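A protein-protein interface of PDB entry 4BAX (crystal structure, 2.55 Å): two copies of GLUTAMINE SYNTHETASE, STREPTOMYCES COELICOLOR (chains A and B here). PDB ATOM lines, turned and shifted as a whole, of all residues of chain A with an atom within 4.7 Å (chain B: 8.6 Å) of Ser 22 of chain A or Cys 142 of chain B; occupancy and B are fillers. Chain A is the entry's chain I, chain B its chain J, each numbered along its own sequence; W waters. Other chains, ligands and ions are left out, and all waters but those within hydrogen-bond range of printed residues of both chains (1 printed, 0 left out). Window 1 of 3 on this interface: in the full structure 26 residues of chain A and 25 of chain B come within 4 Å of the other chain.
The backbone carbonyl oxygen (O) of Gly 138 of chain B lies within hydrogen-bond range of the guanidinium group (NH2) of Arg 21 of chain A (2.8 Å).
The backbone carbonyl oxygen of Cys 142 of chain B sits at hydrogen-bond distance from the backbone NH of Ser 22 of chain A, 2.9 Å away.
O of Tyr 141 of chain B lies close to NH1 of Arg 21 of chain A (2.3 Å).
OG of Ser 22 of chain A is in hydrogen-bond range of OE2 of Glu 7 of chain A, at 2.7 Å.
O of Lys 23 of chain A lies within hydrogen-bond range of N of Tyr 8 of chain A (2.8 Å).
The backbone carbonyl oxygen of Trp 10 of chain A lies within hydrogen-bond range of the backbone NH of Arg 21 of chain A (2.6 Å).
The backbone carbonyl oxygen (O) of Glu 175 of chain B lies close to the backbone NH (N) of Tyr 141 of chain B (3.4 Å).
N of Cys 142 of chain B is in hydrogen-bond range of O of Ala 174 of chain B, 2.9 Å away.
The side-chain carboxylate (OE2) of Glu 175 of chain B sits at hydrogen-bond distance from the side-chain amide nitrogen (ND2) of Asn 173 of chain B.
Gly 139 of chain B touches Arg 21 of chain A (O to NH1, 3.9 Å).
Arg 21 of chain A touches Cys 142 of chain B (CA to O, 3.1 Å).
CB of Lys 23 of chain A touches O of Ile 172 of chain B, at 3.8 Å.
Asn 173 of chain B touches Lys 23 of chain A (CB to CB, 3.7 Å).
CG2 of Val 144 of chain B touches NE1 of Trp 202 of chain A, at 3.9 Å.
Ser 22 of chain A touches one residue of chain B.
Of the printed residues of chain A, Cys 142 of chain B touches Arg 21 (3.1 Å) and Ser 22 (2.9 Å).
Of the printed residues of chain A, Ile 172 of chain B touches Lys 23.
Printed residues of chain A within 4 Å of Tyr 141 of chain B: Arg 21 (2.3 Å).
Of the printed residues of chain B, Lys 23 of chain A touches Ile 172 and Asn 173.
Printed residues of chain B within 4 Å of Trp 202 of chain A: Val 144 (3.9 Å).
The nearest residue of chain B that does not touch Ser 22 of chain A is Gly 143 of chain B (4.7 Å).
The nearest printed residue of chain B that does not touch Arg 21 of chain A is Tyr 140 of chain B (4.5 Å).
Hydrophobic or aromatic side chains of chain B that line the printed part of chain A: Val 144.
Of the 9 printed residues of chain A, 4 touch a printed residue of chain B.
Hydrophobic or aromatic side chains of chain A that line the printed part of chain B: Trp 202.
No position is printed for both chains.
Of the 8 pairs that touch across the chains among the printed residues, none has its exchanged pair printed and touching as well.
Water W1 bridges the backbone carbonyl oxygen (O) of Ser 22 of chain A (2.5 Å) and the backbone NH (N) of Ala 174 of chain B (3.2 Å).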
ATOM      1  N   GLU A   7      -2.959  -6.720  22.827  1.00  0.00           N
ATOM      2  CA  GLU A   7      -1.803  -7.225  23.560  1.00  0.00           C
ATOM      3  C   GLU A   7      -2.300  -8.229  24.594  1.00  0.00           C
ATOM      4  O   GLU A   7      -2.946  -7.851  25.596  1.00  0.00           O
ATOM      5  CB  GLU A   7      -1.025  -6.078  24.230  1.00  0.00           C
ATOM      6  CG  GLU A   7       0.343  -6.466  24.755  1.00  0.00           C
ATOM      7  CD  GLU A   7       1.354  -6.632  23.647  1.00  0.00           C
ATOM      8  OE1 GLU A   7       0.970  -6.364  22.483  1.00  0.00           O
ATOM      9  OE2 GLU A   7       2.505  -7.070  23.925  1.00  0.00           O
ATOM     10  N   TYR A   8      -1.985  -9.500  24.362  1.00  0.00           N
ATOM     11  CA  TYR A   8      -2.433 -10.556  25.249  1.00  0.00           C
ATOM     12  C   TYR A   8      -1.413 -10.707  26.362  1.00  0.00           C
ATOM     13  O   TYR A   8      -0.231 -10.920  26.118  1.00  0.00           O
ATOM     14  CB  TYR A   8      -2.602 -11.882  24.493  1.00  0.00           C
ATOM     15  CG  TYR A   8      -3.946 -12.011  23.800  1.00  0.00           C
ATOM     16  CD1 TYR A   8      -4.428 -10.997  22.975  1.00  0.00           C
ATOM     17  CD2 TYR A   8      -4.749 -13.135  23.984  1.00  0.00           C
ATOM     18  CE1 TYR A   8      -5.657 -11.102  22.346  1.00  0.00           C
ATOM     19  CE2 TYR A   8      -5.992 -13.243  23.354  1.00  0.00           C
ATOM     20  CZ  TYR A   8      -6.432 -12.222  22.539  1.00  0.00           C
ATOM     21  OH  TYR A   8      -7.657 -12.330  21.913  1.00  0.00           O
ATOM     22  N   ILE A   9      -1.885 -10.522  27.590  1.00  0.00           N
ATOM     23  CA  ILE A   9      -1.008 -10.514  28.733  1.00  0.00           C
ATOM     24  C   ILE A   9      -1.379 -11.666  29.645  1.00  0.00           C
ATOM     25  O   ILE A   9      -2.570 -11.928  29.875  1.00  0.00           O
ATOM     26  CB  ILE A   9      -1.096  -9.175  29.504  1.00  0.00           C
ATOM     27  CG1 ILE A   9      -0.617  -8.022  28.633  1.00  0.00           C
ATOM     28  CG2 ILE A   9      -0.305  -9.230  30.808  1.00  0.00           C
ATOM     29  CD1 ILE A   9      -1.210  -6.721  29.030  1.00  0.00           C
ATOM     30  N   TRP A  10      -0.361 -12.379  30.113  1.00  0.00           N
ATOM     31  CA  TRP A  10      -0.575 -13.452  31.062  1.00  0.00           C
ATOM     32  C   TRP A  10       0.554 -13.618  32.091  1.00  0.00           C
ATOM     33  O   TRP A  10       1.601 -12.958  32.028  1.00  0.00           O
ATOM     34  CB  TRP A  10      -0.871 -14.765  30.331  1.00  0.00           C
ATOM     35  CG  TRP A  10       0.300 -15.433  29.633  1.00  0.00           C
ATOM     36  CD1 TRP A  10       1.066 -16.470  30.101  1.00  0.00           C
ATOM     37  CD2 TRP A  10       0.820 -15.113  28.334  1.00  0.00           C
ATOM     38  NE1 TRP A  10       2.030 -16.821  29.163  1.00  0.00           N
ATOM     39  CE2 TRP A  10       1.896 -16.000  28.074  1.00  0.00           C
ATOM     40  CE3 TRP A  10       0.484 -14.160  27.363  1.00  0.00           C
ATOM     41  CZ2 TRP A  10       2.630 -15.952  26.891  1.00  0.00           C
ATOM     42  CZ3 TRP A  10       1.216 -14.121  26.189  1.00  0.00           C
ATOM     43  CH2 TRP A  10       2.272 -15.007  25.962  1.00  0.00           C
ATOM     44  N   LEU A  20       5.165 -11.829  34.262  1.00  0.00           N
ATOM     45  CA  LEU A  20       4.246 -11.395  33.201  1.00  0.00           C
ATOM     46  C   LEU A  20       4.759 -11.717  31.814  1.00  0.00           C
ATOM     47  O   LEU A  20       5.939 -11.552  31.521  1.00  0.00           O
ATOM     48  CB  LEU A  20       3.940  -9.901  33.289  1.00  0.00           C
ATOM     49  CG  LEU A  20       3.063  -9.408  34.431  1.00  0.00           C
ATOM     50  CD1 LEU A  20       3.398  -7.979  34.856  1.00  0.00           C
ATOM     51  CD2 LEU A  20       1.612  -9.523  33.963  1.00  0.00           C
ATOM     52  N   ARG A  21       3.857 -12.135  30.946  1.00  0.00           N
ATOM     53  CA  ARG A  21       4.177 -12.341  29.541  1.00  0.00           C
ATOM     54  C   ARG A  21       3.174 -11.640  28.652  1.00  0.00           C
ATOM     55  O   ARG A  21       2.034 -11.405  29.068  1.00  0.00           O
ATOM     56  CB  ARG A  21       4.245 -13.827  29.208  1.00  0.00           C
ATOM     57  CG  ARG A  21       5.098 -14.601  30.178  1.00  0.00           C
ATOM     58  CD  ARG A  21       6.542 -14.332  29.871  1.00  0.00           C
ATOM     59  NE  ARG A  21       7.432 -15.086  30.736  1.00  0.00           N
ATOM     60  CZ  ARG A  21       8.670 -15.446  30.402  1.00  0.00           C
ATOM     61  NH1 ARG A  21       9.158 -15.177  29.194  1.00  0.00           N
ATOM     62  NH2 ARG A  21       9.404 -16.129  31.264  1.00  0.00           N
ATOM     63  N   SER A  22       3.609 -11.245  27.458  1.00  0.00           N
ATOM     64  CA  SER A  22       2.709 -10.587  26.514  1.00  0.00           C
ATOM     65  C   SER A  22       3.151 -10.800  25.054  1.00  0.00           C
ATOM     66  O   SER A  22       4.344 -11.049  24.779  1.00  0.00           O
ATOM     67  CB  SER A  22       2.530  -9.092  26.861  1.00  0.00           C
ATOM     68  OG  SER A  22       3.431  -8.261  26.142  1.00  0.00           O
ATOM     69  N   LYS A  23       2.158 -10.863  24.159  1.00  0.00           N
ATOM     70  CA  LYS A  23       2.383 -10.755  22.712  1.00  0.00           C
ATOM     71  C   LYS A  23       1.240 -10.027  21.999  1.00  0.00           C
ATOM     72  O   LYS A  23       0.117  -9.955  22.510  1.00  0.00           O
ATOM     73  CB  LYS A  23       2.659 -12.115  22.070  1.00  0.00           C
ATOM     74  CG  LYS A  23       1.711 -13.191  22.582  1.00  0.00           C
ATOM     75  CD  LYS A  23       1.932 -14.513  21.912  1.00  0.00           C
ATOM     76  CE  LYS A  23       1.013 -15.583  22.503  1.00  0.00           C
ATOM     77  NZ  LYS A  23       0.493 -16.525  21.481  1.00  0.00           N
ATOM     78  N   TRP A 202       2.176  -4.558  34.662  1.00  0.00           N
ATOM     79  CA  TRP A 202       2.645  -4.710  33.305  1.00  0.00           C
ATOM     80  C   TRP A 202       2.908  -3.329  32.685  1.00  0.00           C
ATOM     81  O   TRP A 202       3.893  -3.117  31.966  1.00  0.00           O
ATOM     82  CB  TRP A 202       1.646  -5.519  32.484  1.00  0.00           C
ATOM     83  CG  TRP A 202       2.109  -5.748  31.113  1.00  0.00           C
ATOM     84  CD1 TRP A 202       2.847  -6.804  30.661  1.00  0.00           C
ATOM     85  CD2 TRP A 202       1.910  -4.881  29.996  1.00  0.00           C
ATOM     86  NE1 TRP A 202       3.103  -6.656  29.322  1.00  0.00           N
ATOM     87  CE2 TRP A 202       2.545  -5.479  28.888  1.00  0.00           C
ATOM     88  CE3 TRP A 202       1.246  -3.660  29.818  1.00  0.00           C
ATOM     89  CZ2 TRP A 202       2.529  -4.899  27.610  1.00  0.00           C
ATOM     90  CZ3 TRP A 202       1.233  -3.086  28.553  1.00  0.00           C
ATOM     91  CH2 TRP A 202       1.871  -3.706  27.466  1.00  0.00           C
ATOM     92  N   GLY B 138      15.114 -17.446  29.206  1.00  0.00           N
ATOM     93  CA  GLY B 138      13.961 -17.780  30.025  1.00  0.00           C
ATOM     94  C   GLY B 138      13.039 -16.599  30.245  1.00  0.00           C
ATOM     95  O   GLY B 138      11.819 -16.716  30.066  1.00  0.00           O
ATOM     96  N   GLY B 139      13.614 -15.435  30.526  1.00  0.00           N
ATOM     97  CA  GLY B 139      12.801 -14.265  30.757  1.00  0.00           C
ATOM     98  C   GLY B 139      12.656 -13.357  29.550  1.00  0.00           C
ATOM     99  O   GLY B 139      11.870 -12.422  29.602  1.00  0.00           O
ATOM    100  N   TYR B 140      13.392 -13.612  28.466  1.00  0.00           N
ATOM    101  CA  TYR B 140      13.271 -12.758  27.268  1.00  0.00           C
ATOM    102  C   TYR B 140      12.004 -12.970  26.433  1.00  0.00           C
ATOM    103  O   TYR B 140      11.430 -12.035  25.869  1.00  0.00           O
ATOM    104  CB  TYR B 140      14.541 -12.825  26.396  1.00  0.00           C
ATOM    105  CG  TYR B 140      15.796 -12.745  27.227  1.00  0.00           C
ATOM    106  CD1 TYR B 140      16.156 -11.557  27.852  1.00  0.00           C
ATOM    107  CD2 TYR B 140      16.619 -13.858  27.406  1.00  0.00           C
ATOM    108  CE1 TYR B 140      17.306 -11.469  28.650  1.00  0.00           C
ATOM    109  CE2 TYR B 140      17.784 -13.788  28.201  1.00  0.00           C
ATOM    110  CZ  TYR B 140      18.126 -12.584  28.825  1.00  0.00           C
ATOM    111  OH  TYR B 140      19.262 -12.484  29.616  1.00  0.00           O
ATOM    112  N   TYR B 141      11.572 -14.213  26.377  1.00  0.00           N
ATOM    113  CA  TYR B 141      10.527 -14.606  25.461  1.00  0.00           C
ATOM    114  C   TYR B 141       9.182 -14.080  25.926  1.00  0.00           C
ATOM    115  O   TYR B 141       8.774 -14.349  27.057  1.00  0.00           O
ATOM    116  CB  TYR B 141      10.508 -16.116  25.347  1.00  0.00           C
ATOM    117  CG  TYR B 141       9.311 -16.662  24.617  1.00  0.00           C
ATOM    118  CD1 TYR B 141       9.297 -16.736  23.220  1.00  0.00           C
ATOM    119  CD2 TYR B 141       8.202 -17.133  25.311  1.00  0.00           C
ATOM    120  CE1 TYR B 141       8.207 -17.259  22.532  1.00  0.00           C
ATOM    121  CE2 TYR B 141       7.101 -17.664  24.624  1.00  0.00           C
ATOM    122  CZ  TYR B 141       7.112 -17.723  23.234  1.00  0.00           C
ATOM    123  OH  TYR B 141       6.030 -18.246  22.546  1.00  0.00           O
ATOM    124  N   CYS B 142       8.542 -13.274  25.077  1.00  0.00           N
ATOM    125  CA  CYS B 142       7.261 -12.650  25.422  1.00  0.00           C
ATOM    126  C   CYS B 142       7.388 -11.827  26.694  1.00  0.00           C
ATOM    127  O   CYS B 142       6.444 -11.752  27.475  1.00  0.00           O
ATOM    128  CB  CYS B 142       6.151 -13.708  25.562  1.00  0.00           C
ATOM    129  SG  CYS B 142       5.728 -14.523  23.987  1.00  0.00           S
ATOM    130  N   GLY B 143       8.587 -11.257  26.894  1.00  0.00           N
ATOM    131  CA  GLY B 143       8.963 -10.530  28.103  1.00  0.00           C
ATOM    132  C   GLY B 143       8.523  -9.085  28.224  1.00  0.00           C
ATOM    133  O   GLY B 143       7.928  -8.520  27.319  1.00  0.00           O
ATOM    134  N   VAL B 144       8.818  -8.477  29.362  1.00  0.00           N
ATOM    135  CA  VAL B 144       8.554  -7.062  29.558  1.00  0.00           C
ATOM    136  C   VAL B 144       9.633  -6.505  30.476  1.00  0.00           C
ATOM    137  O   VAL B 144      10.180  -7.257  31.297  1.00  0.00           O
ATOM    138  CB  VAL B 144       7.130  -6.839  30.134  1.00  0.00           C
ATOM    139  CG1 VAL B 144       7.016  -7.403  31.549  1.00  0.00           C
ATOM    140  CG2 VAL B 144       6.731  -5.366  30.087  1.00  0.00           C
ATOM    141  N   GLY B 145       9.983  -5.230  30.314  1.00  0.00           N
ATOM    142  CA  GLY B 145      10.997  -4.605  31.159  1.00  0.00           C
ATOM    143  C   GLY B 145      12.362  -4.396  30.530  1.00  0.00           C
ATOM    144  O   GLY B 145      12.799  -5.213  29.712  1.00  0.00           O
ATOM    145  N   GLU B 148      15.010  -7.222  30.225  1.00  0.00           N
ATOM    146  CA  GLU B 148      14.804  -8.329  29.304  1.00  0.00           C
ATOM    147  C   GLU B 148      14.326  -8.011  27.870  1.00  0.00           C
ATOM    148  O   GLU B 148      14.219  -8.922  27.047  1.00  0.00           O
ATOM    149  CB  GLU B 148      13.855  -9.353  29.953  1.00  0.00           C
ATOM    150  CG  GLU B 148      14.520 -10.187  31.058  1.00  0.00           C
ATOM    151  CD  GLU B 148      13.597 -10.517  32.237  1.00  0.00           C
ATOM    152  OE1 GLU B 148      12.591  -9.808  32.489  1.00  0.00           O
ATOM    153  OE2 GLU B 148      13.904 -11.500  32.936  1.00  0.00           O
ATOM    154  N   ILE B 149      14.007  -6.752  27.586  1.00  0.00           N
ATOM    155  CA  ILE B 149      13.469  -6.353  26.281  1.00  0.00           C
ATOM    156  C   ILE B 149      14.345  -5.320  25.611  1.00  0.00           C
ATOM    157  O   ILE B 149      14.654  -4.292  26.209  1.00  0.00           O
ATOM    158  CB  ILE B 149      12.001  -5.851  26.378  1.00  0.00           C
ATOM    159  CG1 ILE B 149      11.073  -7.010  26.763  1.00  0.00           C
ATOM    160  CG2 ILE B 149      11.538  -5.225  25.062  1.00  0.00           C
ATOM    161  CD1 ILE B 149      11.003  -8.135  25.739  1.00  0.00           C
ATOM    162  N   ARG B 152      12.231  -2.695  21.406  1.00  0.00           N
ATOM    163  CA  ARG B 152      10.783  -2.621  21.256  1.00  0.00           C
ATOM    164  C   ARG B 152      10.313  -1.427  20.454  1.00  0.00           C
ATOM    165  O   ARG B 152       9.365  -1.542  19.670  1.00  0.00           O
ATOM    166  CB  ARG B 152      10.047  -2.634  22.595  1.00  0.00           C
ATOM    167  CG  ARG B 152       8.720  -3.343  22.493  1.00  0.00           C
ATOM    168  CD  ARG B 152       7.721  -2.831  23.509  1.00  0.00           C
ATOM    169  NE  ARG B 152       7.925  -3.455  24.812  1.00  0.00           N
ATOM    170  CZ  ARG B 152       7.491  -4.674  25.120  1.00  0.00           C
ATOM    171  NH1 ARG B 152       6.861  -5.409  24.208  1.00  0.00           N
ATOM    172  NH2 ARG B 152       7.716  -5.174  26.334  1.00  0.00           N
ATOM    173  N   GLU B 156       7.880  -1.788  17.320  1.00  0.00           N
ATOM    174  CA  GLU B 156       6.595  -1.066  17.247  1.00  0.00           C
ATOM    175  C   GLU B 156       6.494  -0.165  16.042  1.00  0.00           C
ATOM    176  O   GLU B 156       5.434  -0.105  15.403  1.00  0.00           O
ATOM    177  CB  GLU B 156       6.336  -0.236  18.517  1.00  0.00           C
ATOM    178  CG  GLU B 156       6.119  -1.025  19.801  1.00  0.00           C
ATOM    179  CD  GLU B 156       4.711  -1.569  19.929  1.00  0.00           C
ATOM    180  OE1 GLU B 156       3.785  -1.025  19.290  1.00  0.00           O
ATOM    181  OE2 GLU B 156       4.532  -2.579  20.632  1.00  0.00           O
ATOM    182  N   ILE B 172       2.964 -10.052  16.358  1.00  0.00           N
ATOM    183  CA  ILE B 172       4.388  -9.958  16.596  1.00  0.00           C
ATOM    184  C   ILE B 172       4.653 -10.462  18.001  1.00  0.00           C
ATOM    185  O   ILE B 172       3.741 -10.442  18.849  1.00  0.00           O
ATOM    186  CB  ILE B 172       4.910  -8.512  16.452  1.00  0.00           C
ATOM    187  CG1 ILE B 172       4.117  -7.600  17.394  1.00  0.00           C
ATOM    188  CG2 ILE B 172       4.716  -7.994  15.021  1.00  0.00           C
ATOM    189  CD1 ILE B 172       4.905  -6.442  18.003  1.00  0.00           C
ATOM    190  N   ASN B 173       5.863 -10.971  18.239  1.00  0.00           N
ATOM    191  CA  ASN B 173       6.265 -11.304  19.608  1.00  0.00           C
ATOM    192  C   ASN B 173       7.775 -11.258  19.821  1.00  0.00           C
ATOM    193  O   ASN B 173       8.552 -11.378  18.853  1.00  0.00           O
ATOM    194  CB  ASN B 173       5.719 -12.670  20.049  1.00  0.00           C
ATOM    195  CG  ASN B 173       6.350 -13.835  19.278  1.00  0.00           C
ATOM    196  OD1 ASN B 173       5.912 -14.188  18.176  1.00  0.00           O
ATOM    197  ND2 ASN B 173       7.399 -14.424  19.856  1.00  0.00           N
ATOM    198  N   ALA B 174       8.175 -11.111  21.091  1.00  0.00           N
ATOM    199  CA  ALA B 174       9.586 -11.190  21.481  1.00  0.00           C
ATOM    200  C   ALA B 174       9.995 -12.648  21.612  1.00  0.00           C
ATOM    201  O   ALA B 174       9.280 -13.450  22.236  1.00  0.00           O
ATOM    202  CB  ALA B 174       9.812 -10.474  22.783  1.00  0.00           C
ATOM    203  N   GLU B 175      11.159 -12.990  21.074  1.00  0.00           N
ATOM    204  CA  GLU B 175      11.584 -14.385  21.069  1.00  0.00           C
ATOM    205  C   GLU B 175      12.476 -14.773  22.246  1.00  0.00           C
ATOM    206  O   GLU B 175      12.729 -13.964  23.148  1.00  0.00           O
ATOM    207  CB  GLU B 175      12.209 -14.767  19.737  1.00  0.00           C
ATOM    208  CG  GLU B 175      11.211 -15.367  18.746  1.00  0.00           C
ATOM    209  CD  GLU B 175      10.625 -16.711  19.232  1.00  0.00           C
ATOM    210  OE1 GLU B 175      11.408 -17.535  19.792  1.00  0.00           O
ATOM    211  OE2 GLU B 175       9.412 -16.976  18.989  1.00  0.00           O
ATOM    212  N   VAL B 176      12.899 -16.036  22.229  1.00  0.00           N
ATOM    213  CA  VAL B 176      13.610 -16.674  23.340  1.00  0.00           C
ATOM    214  C   VAL B 176      14.958 -16.021  23.665  1.00  0.00           C
ATOM    215  O   VAL B 176      15.262 -15.772  24.832  1.00  0.00           O
ATOM    216  CB  VAL B 176      13.792 -18.200  23.060  1.00  0.00           C
ATOM    217  CG1 VAL B 176      14.690 -18.865  24.116  1.00  0.00           C
ATOM    218  CG2 VAL B 176      12.402 -18.895  22.953  1.00  0.00           C
ATOM    219  N   MET B 177      15.704 -15.669  22.619  1.00  0.00           N
ATOM    220  CA  MET B 177      16.971 -14.946  22.723  1.00  0.00           C
ATOM    221  C   MET B 177      16.770 -13.438  22.932  1.00  0.00           C
ATOM    222  O   MET B 177      15.847 -12.859  22.362  1.00  0.00           O
ATOM    223  CB  MET B 177      17.800 -15.188  21.468  1.00  0.00           C
ATOM    224  CG  MET B 177      19.239 -14.764  21.625  1.00  0.00           C
ATOM    225  SD  MET B 177      20.197 -14.846  20.101  1.00  0.00           S
ATOM    226  CE  MET B 177      21.303 -13.470  20.386  1.00  0.00           C
ATOM    227  N   GLN B 180      15.852 -10.749  20.207  1.00  0.00           N
ATOM    228  CA  GLN B 180      15.270 -11.531  19.127  1.00  0.00           C
ATOM    229  C   GLN B 180      13.751 -11.400  19.121  1.00  0.00           C
ATOM    230  O   GLN B 180      13.099 -11.491  20.175  1.00  0.00           O
ATOM    231  CB  GLN B 180      15.679 -12.987  19.271  1.00  0.00           C
ATOM    232  CG  GLN B 180      15.618 -13.807  17.991  1.00  0.00           C
ATOM    233  CD  GLN B 180      16.186 -15.185  18.194  1.00  0.00           C
ATOM    234  OE1 GLN B 180      15.619 -16.005  18.918  1.00  0.00           O
ATOM    235  NE2 GLN B 180      17.324 -15.453  17.559  1.00  0.00           N
ATOM    236  N   TRP B 181      13.198 -11.227  17.922  1.00  0.00           N
ATOM    237  CA  TRP B 181      11.777 -10.927  17.735  1.00  0.00           C
ATOM    238  C   TRP B 181      11.161 -11.697  16.575  1.00  0.00           C
ATOM    239  O   TRP B 181      11.874 -12.290  15.754  1.00  0.00           O
ATOM    240  CB  TRP B 181      11.584  -9.430  17.480  1.00  0.00           C
ATOM    241  CG  TRP B 181      11.922  -8.546  18.640  1.00  0.00           C
ATOM    242  CD1 TRP B 181      13.160  -8.054  18.974  1.00  0.00           C
ATOM    243  CD2 TRP B 181      11.015  -8.050  19.634  1.00  0.00           C
ATOM    244  NE1 TRP B 181      13.069  -7.271  20.106  1.00  0.00           N
ATOM    245  CE2 TRP B 181      11.766  -7.257  20.530  1.00  0.00           C
ATOM    246  CE3 TRP B 181       9.641  -8.192  19.848  1.00  0.00           C
ATOM    247  CZ2 TRP B 181      11.188  -6.613  21.623  1.00  0.00           C
ATOM    248  CZ3 TRP B 181       9.067  -7.550  20.943  1.00  0.00           C
ATOM    249  CH2 TRP B 181       9.840  -6.769  21.813  1.00  0.00           C
ATOM    250  N   GLN B 184       4.408 -12.309  12.148  1.00  0.00           N
ATOM    251  CA  GLN B 184       3.744 -13.339  11.351  1.00  0.00           C
ATOM    252  C   GLN B 184       3.022 -12.699  10.164  1.00  0.00           C
ATOM    253  O   GLN B 184       2.223 -11.766  10.322  1.00  0.00           O
ATOM    254  CB  GLN B 184       2.740 -14.130  12.201  1.00  0.00           C
ATOM    255  CG  GLN B 184       3.352 -14.828  13.397  1.00  0.00           C
ATOM    256  CD  GLN B 184       2.899 -14.203  14.700  1.00  0.00           C
ATOM    257  OE1 GLN B 184       1.761 -13.727  14.813  1.00  0.00           O
ATOM    258  NE2 GLN B 184       3.802 -14.150  15.675  1.00  0.00           N
HETATM  259  O   HOH W   1       6.100 -10.093  23.278  1.00  0.00           O
